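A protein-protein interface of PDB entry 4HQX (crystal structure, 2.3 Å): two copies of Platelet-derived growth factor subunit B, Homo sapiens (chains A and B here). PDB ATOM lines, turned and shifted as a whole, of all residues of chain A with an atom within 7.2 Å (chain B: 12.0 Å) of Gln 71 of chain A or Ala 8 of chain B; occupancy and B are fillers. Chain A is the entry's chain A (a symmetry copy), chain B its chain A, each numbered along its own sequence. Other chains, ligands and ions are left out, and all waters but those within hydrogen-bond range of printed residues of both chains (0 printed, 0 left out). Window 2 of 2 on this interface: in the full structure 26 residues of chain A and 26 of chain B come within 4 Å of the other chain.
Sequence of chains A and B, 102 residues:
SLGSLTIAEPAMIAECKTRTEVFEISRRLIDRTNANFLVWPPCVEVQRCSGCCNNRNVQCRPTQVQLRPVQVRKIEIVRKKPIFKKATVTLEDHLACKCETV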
ATOM      1  N   TRP A  40      18.387  -0.743  11.480  1.00  0.00           N
ATOM      2  CA  TRP A  40      19.550  -0.327  12.234  1.00  0.00           C
ATOM      3  C   TRP A  40      19.107   0.267  13.551  1.00  0.00           C
ATOM      4  O   TRP A  40      18.142   1.039  13.589  1.00  0.00           O
ATOM      5  CB  TRP A  40      20.370   0.688  11.456  1.00  0.00           C
ATOM      6  CG  TRP A  40      21.682   0.958  12.133  1.00  0.00           C
ATOM      7  CD1 TRP A  40      21.985   1.972  13.048  1.00  0.00           C
ATOM      8  CD2 TRP A  40      22.910   0.169  12.007  1.00  0.00           C
ATOM      9  NE1 TRP A  40      23.286   1.875  13.457  1.00  0.00           N
ATOM     10  CE2 TRP A  40      23.895   0.809  12.875  1.00  0.00           C
ATOM     11  CE3 TRP A  40      23.278  -0.949  11.270  1.00  0.00           C
ATOM     12  CZ2 TRP A  40      25.186   0.326  12.998  1.00  0.00           C
ATOM     13  CZ3 TRP A  40      24.586  -1.431  11.398  1.00  0.00           C
ATOM     14  CH2 TRP A  40      25.517  -0.804  12.245  1.00  0.00           C
ATOM     15  N   PRO A  41      19.800  -0.082  14.656  1.00  0.00           N
ATOM     16  CA  PRO A  41      20.950  -1.008  14.768  1.00  0.00           C
ATOM     17  C   PRO A  41      20.526  -2.494  14.766  1.00  0.00           C
ATOM     18  O   PRO A  41      19.343  -2.785  14.984  1.00  0.00           O
ATOM     19  CB  PRO A  41      21.556  -0.631  16.119  1.00  0.00           C
ATOM     20  CG  PRO A  41      20.385  -0.169  16.925  1.00  0.00           C
ATOM     21  CD  PRO A  41      19.395   0.453  15.970  1.00  0.00           C
ATOM     22  N   ARG A  68      10.274  -2.507  27.347  1.00  0.00           N
ATOM     23  CA  ARG A  68      10.960  -1.274  26.977  1.00  0.00           C
ATOM     24  C   ARG A  68      10.913  -1.119  25.458  1.00  0.00           C
ATOM     25  O   ARG A  68      11.525  -1.897  24.721  1.00  0.00           O
ATOM     26  CB  ARG A  68      12.395  -1.282  27.499  1.00  0.00           C
ATOM     27  CG  ARG A  68      13.194  -0.031  27.175  1.00  0.00           C
ATOM     28  CD  ARG A  68      14.499   0.037  27.963  1.00  0.00           C
ATOM     29  NE  ARG A  68      15.258  -1.213  27.884  1.00  0.00           N
ATOM     30  CZ  ARG A  68      16.308  -1.428  27.091  1.00  0.00           C
ATOM     31  NH1 ARG A  68      16.759  -0.476  26.280  1.00  0.00           N
ATOM     32  NH2 ARG A  68      16.916  -2.608  27.110  1.00  0.00           N
ATOM     33  N   PRO A  69      10.143  -0.134  24.975  1.00  0.00           N
ATOM     34  CA  PRO A  69      10.076   0.045  23.532  1.00  0.00           C
ATOM     35  C   PRO A  69      11.248   0.891  23.053  1.00  0.00           C
ATOM     36  O   PRO A  69      11.631   1.868  23.718  1.00  0.00           O
ATOM     37  CB  PRO A  69       8.739   0.779  23.325  1.00  0.00           C
ATOM     38  CG  PRO A  69       8.207   1.117  24.696  1.00  0.00           C
ATOM     39  CD  PRO A  69       9.296   0.836  25.693  1.00  0.00           C
ATOM     40  N   VAL A  70      11.844   0.485  21.936  1.00  0.00           N
ATOM     41  CA  VAL A  70      12.883   1.288  21.288  1.00  0.00           C
ATOM     42  C   VAL A  70      12.587   1.471  19.801  1.00  0.00           C
ATOM     43  O   VAL A  70      11.998   0.601  19.144  1.00  0.00           O
ATOM     44  CB  VAL A  70      14.323   0.723  21.469  1.00  0.00           C
ATOM     45  CG1 VAL A  70      14.763   0.797  22.928  1.00  0.00           C
ATOM     46  CG2 VAL A  70      14.458  -0.690  20.891  1.00  0.00           C
ATOM     47  N   GLN A  71      13.029   2.614  19.297  1.00  0.00           N
ATOM     48  CA  GLN A  71      12.785   3.047  17.937  1.00  0.00           C
ATOM     49  C   GLN A  71      13.993   2.631  17.122  1.00  0.00           C
ATOM     50  O   GLN A  71      15.111   3.056  17.412  1.00  0.00           O
ATOM     51  CB  GLN A  71      12.660   4.575  17.937  1.00  0.00           C
ATOM     52  CG  GLN A  71      11.983   5.189  16.725  1.00  0.00           C
ATOM     53  CD  GLN A  71      11.524   6.623  16.981  1.00  0.00           C
ATOM     54  OE1 GLN A  71      12.340   7.552  17.066  1.00  0.00           O
ATOM     55  NE2 GLN A  71      10.210   6.810  17.098  1.00  0.00           N
ATOM     56  N   VAL A  72      13.782   1.782  16.126  1.00  0.00           N
ATOM     57  CA  VAL A  72      14.866   1.428  15.227  1.00  0.00           C
ATOM     58  C   VAL A  72      14.656   2.073  13.865  1.00  0.00           C
ATOM     59  O   VAL A  72      13.523   2.284  13.433  1.00  0.00           O
ATOM     60  CB  VAL A  72      15.049  -0.102  15.064  1.00  0.00           C
ATOM     61  CG1 VAL A  72      15.229  -0.763  16.420  1.00  0.00           C
ATOM     62  CG2 VAL A  72      13.882  -0.720  14.319  1.00  0.00           C
ATOM     63  N   ARG A  73      15.755   2.387  13.199  1.00  0.00           N
ATOM     64  CA  ARG A  73      15.696   2.921  11.850  1.00  0.00           C
ATOM     65  C   ARG A  73      15.432   1.813  10.841  1.00  0.00           C
ATOM     66  O   ARG A  73      15.992   0.731  10.950  1.00  0.00           O
ATOM     67  CB  ARG A  73      16.987   3.671  11.544  1.00  0.00           C
ATOM     68  CG  ARG A  73      16.925   5.063  12.126  1.00  0.00           C
ATOM     69  CD  ARG A  73      18.215   5.553  12.737  1.00  0.00           C
ATOM     70  NE  ARG A  73      18.134   7.013  12.796  1.00  0.00           N
ATOM     71  CZ  ARG A  73      18.931   7.855  12.141  1.00  0.00           C
ATOM     72  NH1 ARG A  73      18.724   9.151  12.264  1.00  0.00           N
ATOM     73  NH2 ARG A  73      19.942   7.412  11.387  1.00  0.00           N
ATOM     74  N   LYS A  85      11.801   4.820   7.135  1.00  0.00           N
ATOM     75  CA  LYS A  85      10.726   4.565   8.084  1.00  0.00           C
ATOM     76  C   LYS A  85      11.323   4.412   9.478  1.00  0.00           C
ATOM     77  O   LYS A  85      12.545   4.329   9.642  1.00  0.00           O
ATOM     78  CB  LYS A  85       9.981   3.287   7.708  1.00  0.00           C
ATOM     79  CG  LYS A  85       8.765   3.465   6.808  1.00  0.00           C
ATOM     80  CD  LYS A  85       7.746   2.372   7.145  1.00  0.00           C
ATOM     81  CE  LYS A  85       6.362   2.589   6.537  1.00  0.00           C
ATOM     82  NZ  LYS A  85       6.342   2.410   5.057  1.00  0.00           N
ATOM     83  N   LYS A  86      10.457   4.389  10.481  1.00  0.00           N
ATOM     84  CA  LYS A  86      10.859   4.072  11.844  1.00  0.00           C
ATOM     85  C   LYS A  86      10.000   2.922  12.347  1.00  0.00           C
ATOM     86  O   LYS A  86       8.800   2.882  12.092  1.00  0.00           O
ATOM     87  CB  LYS A  86      10.700   5.285  12.757  1.00  0.00           C
ATOM     88  CG  LYS A  86      11.667   6.409  12.448  1.00  0.00           C
ATOM     89  CD  LYS A  86      11.562   7.540  13.453  1.00  0.00           C
ATOM     90  CE  LYS A  86      12.482   8.681  13.058  1.00  0.00           C
ATOM     91  NZ  LYS A  86      12.608   9.703  14.130  1.00  0.00           N
ATOM     92  N   ALA A  87      10.616   1.974  13.039  1.00  0.00           N
ATOM     93  CA  ALA A  87       9.863   0.878  13.634  1.00  0.00           C
ATOM     94  C   ALA A  87      10.110   0.847  15.135  1.00  0.00           C
ATOM     95  O   ALA A  87      11.154   1.290  15.613  1.00  0.00           O
ATOM     96  CB  ALA A  87      10.228  -0.447  12.985  1.00  0.00           C
ATOM     97  N   THR A  88       9.125   0.354  15.874  1.00  0.00           N
ATOM     98  CA  THR A  88       9.233   0.248  17.317  1.00  0.00           C
ATOM     99  C   THR A  88       9.421  -1.227  17.684  1.00  0.00           C
ATOM    100  O   THR A  88       8.607  -2.067  17.318  1.00  0.00           O
ATOM    101  CB  THR A  88       7.991   0.857  18.012  1.00  0.00           C
ATOM    102  OG1 THR A  88       7.819   2.218  17.581  1.00  0.00           O
ATOM    103  CG2 THR A  88       8.144   0.822  19.538  1.00  0.00           C
ATOM    104  N   VAL A  89      10.519  -1.536  18.366  1.00  0.00           N
ATOM    105  CA  VAL A  89      10.748  -2.883  18.900  1.00  0.00           C
ATOM    106  C   VAL A  89      10.575  -2.839  20.416  1.00  0.00           C
ATOM    107  O   VAL A  89      11.154  -1.987  21.090  1.00  0.00           O
ATOM    108  CB  VAL A  89      12.148  -3.434  18.542  1.00  0.00           C
ATOM    109  CG1 VAL A  89      12.369  -4.791  19.193  1.00  0.00           C
ATOM    110  CG2 VAL A  89      12.304  -3.560  17.033  1.00  0.00           C
ATOM    111  N   ILE B   7       7.236   7.267  25.825  1.00  0.00           N
ATOM    112  CA  ILE B   7       8.392   7.579  24.934  1.00  0.00           C
ATOM    113  C   ILE B   7       9.151   6.314  24.533  1.00  0.00           C
ATOM    114  O   ILE B   7       9.427   5.446  25.372  1.00  0.00           O
ATOM    115  CB  ILE B   7       9.377   8.564  25.594  1.00  0.00           C
ATOM    116  N   ALA B   8       9.469   6.213  23.241  1.00  0.00           N
ATOM    117  CA  ALA B   8      10.328   5.148  22.730  1.00  0.00           C
ATOM    118  C   ALA B   8      11.666   5.739  22.301  1.00  0.00           C
ATOM    119  O   ALA B   8      11.754   6.436  21.293  1.00  0.00           O
ATOM    120  CB  ALA B   8       9.658   4.417  21.582  1.00  0.00           C
ATOM    121  N   GLU B   9      12.698   5.466  23.094  1.00  0.00           N
ATOM    122  CA  GLU B   9      14.045   5.976  22.855  1.00  0.00           C
ATOM    123  C   GLU B   9      14.659   5.377  21.594  1.00  0.00           C
ATOM    124  O   GLU B   9      14.323   4.253  21.215  1.00  0.00           O
ATOM    125  CB  GLU B   9      14.954   5.656  24.051  1.00  0.00           C
ATOM    126  CG  GLU B   9      14.416   6.098  25.406  1.00  0.00           C
ATOM    127  CD  GLU B   9      14.140   7.591  25.475  1.00  0.00           C
ATOM    128  OE1 GLU B   9      12.979   7.973  25.757  1.00  0.00           O
ATOM    129  OE2 GLU B   9      15.079   8.381  25.238  1.00  0.00           O
ATOM    130  N   PRO B  10      15.566   6.119  20.940  1.00  0.00           N
ATOM    131  CA  PRO B  10      16.308   5.497  19.848  1.00  0.00           C
ATOM    132  C   PRO B  10      17.057   4.280  20.380  1.00  0.00           C
ATOM    133  O   PRO B  10      17.673   4.357  21.447  1.00  0.00           O
ATOM    134  CB  PRO B  10      17.317   6.577  19.428  1.00  0.00           C
ATOM    135  CG  PRO B  10      16.782   7.854  19.964  1.00  0.00           C
ATOM    136  CD  PRO B  10      15.969   7.514  21.176  1.00  0.00           C
ATOM    137  N   ALA B  11      16.980   3.167  19.660  1.00  0.00           N
ATOM    138  CA  ALA B  11      17.782   1.996  19.970  1.00  0.00           C
ATOM    139  C   ALA B  11      19.246   2.366  19.779  1.00  0.00           C
ATOM    140  O   ALA B  11      19.573   3.088  18.843  1.00  0.00           O
ATOM    141  CB  ALA B  11      17.399   0.850  19.066  1.00  0.00           C
ATOM    142  N   MET B  12      20.107   1.923  20.695  1.00  0.00           N
ATOM    143  CA  MET B  12      21.553   2.139  20.591  1.00  0.00           C
ATOM    144  C   MET B  12      22.247   0.816  20.317  1.00  0.00           C
ATOM    145  O   MET B  12      21.838  -0.232  20.826  1.00  0.00           O
ATOM    146  CB  MET B  12      22.123   2.742  21.880  1.00  0.00           C
ATOM    147  CG  MET B  12      21.459   4.026  22.356  1.00  0.00           C
ATOM    148  SD  MET B  12      21.703   5.369  21.183  1.00  0.00           S
ATOM    149  CE  MET B  12      23.497   5.464  21.100  1.00  0.00           C
ATOM    150  N   ILE B  13      23.301   0.859  19.512  1.00  0.00           N
ATOM    151  CA  ILE B  13      23.984  -0.369  19.141  1.00  0.00           C
ATOM    152  C   ILE B  13      24.736  -0.995  20.340  1.00  0.00           C
ATOM    153  O   ILE B  13      25.419  -0.299  21.095  1.00  0.00           O
ATOM    154  CB  ILE B  13      24.905  -0.179  17.906  1.00  0.00           C
ATOM    155  CG1 ILE B  13      25.370  -1.555  17.403  1.00  0.00           C
ATOM    156  CG2 ILE B  13      26.059   0.781  18.205  1.00  0.00           C
ATOM    157  CD1 ILE B  13      26.006  -1.567  16.039  1.00  0.00           C
ATOM    158  N   ALA B  14      24.586  -2.304  20.518  1.00  0.00           N
ATOM    159  CA  ALA B  14      25.442  -3.048  21.431  1.00  0.00           C
ATOM    160  C   ALA B  14      26.770  -3.180  20.709  1.00  0.00           C
ATOM    161  O   ALA B  14      26.943  -4.045  19.842  1.00  0.00           O
ATOM    162  CB  ALA B  14      24.855  -4.416  21.739  1.00  0.00           C
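The backbone NH of Gln 71 of chain A lies within hydrogen-bond range of the backbone carbonyl oxygen of Glu 9 of chain B.
The backbone NH (N) of Ala 11 of chain B sits at hydrogen-bond distance from the backbone carbonyl oxygen (O) of Gln 71 of chain A (2.9 Å).
The backbone NH (N) of Val 72 of chain A sits at hydrogen-bond distance from the backbone carbonyl oxygen (O) of Ala 87 of chain A (2.7 Å).
N of Arg 73 of chain A lies within hydrogen-bond range of O of Trp 40 of chain A, at 2.8 Å.
The backbone NH of Val 70 of chain A lies within hydrogen-bond range of the backbone carbonyl oxygen of Val 89 of chain A (2.7 Å).
Ile 13 of chain B touches Trp 40 of chain A.
CD of Pro 41 of chain A touches CB of Ala 11 of chain B, at 3.7 Å.
Met 12 of chain B touches Pro 41 of chain A (C to CG, 3.99 Å).
CB of Pro 41 of chain A touches CB of Ile 13 of chain B (3.8 Å).
Pro 69 of chain A touches Ala 8 of chain B.
Glu 9 of chain B touches Pro 69 of chain A.
O of Glu 9 of chain B touches CA of Val 70 of chain A, 3.3 Å away.
CB of Ala 11 of chain B touches CG2 of Val 70 of chain A, at 3.8 Å.
CB of Gln 71 of chain A touches O of Ala 8 of chain B, 3.9 Å away.
CB of Ala 11 of chain B touches CG1 of Val 72 of chain A (3.8 Å).
Of chain B, only Ala 8, Glu 9, Pro 10 and Ala 11 come within 4 Å of Gln 71 of chain A.
Of chain B, only Ala 8 and Glu 9 come within 4 Å of Pro 69 of chain A.
Val 72 of chain A touches just one residue of chain B: Ala 11.
Ala 87 of chain A touches none of the printed residues of chain B.
Printed residues of chain A within 4 Å of Pro 10 of chain B: Gln 71.
Printed residues of chain B within 4 Å of Trp 40 of chain A: Ile 13 (3.7 Å).
Printed residues of chain A within 4 Å of Met 12 of chain B: Pro 41.
Of the printed residues of chain A, Ile 13 of chain B touches Trp 40 and Pro 41.
Of the printed residues of chain A, Ala 11 of chain B touches Pro 41 (3.7 Å), Val 70 (3.8 Å), Gln 71 (2.9 Å) and Val 72 (3.8 Å).
Lys 85 of chain A touches none of the printed residues of chain B.
Printed residues of chain A that touch a printed residue of chain B: Trp 40, Pro 41, Pro 69, Val 70, Gln 71 and Val 72.
Of the 8 printed residues of chain B, 6 touch a printed residue of chain A.
Hydrophobic or aromatic side chains of chain B within 4 Å of the printed part of chain A: Ala 8, Ala 11 and Ile 13.
Among the printed residues, 13 pairs touch across the chains.
Among the printed residues, no Asp or Glu carboxylate lies within 4 Å of a Lys or Arg side-chain nitrogen of the other chain.
No position is printed for both chains.
Of the 13 pairs that touch across the chains among the printed residues, none has its exchanged pair printed and touching as well.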
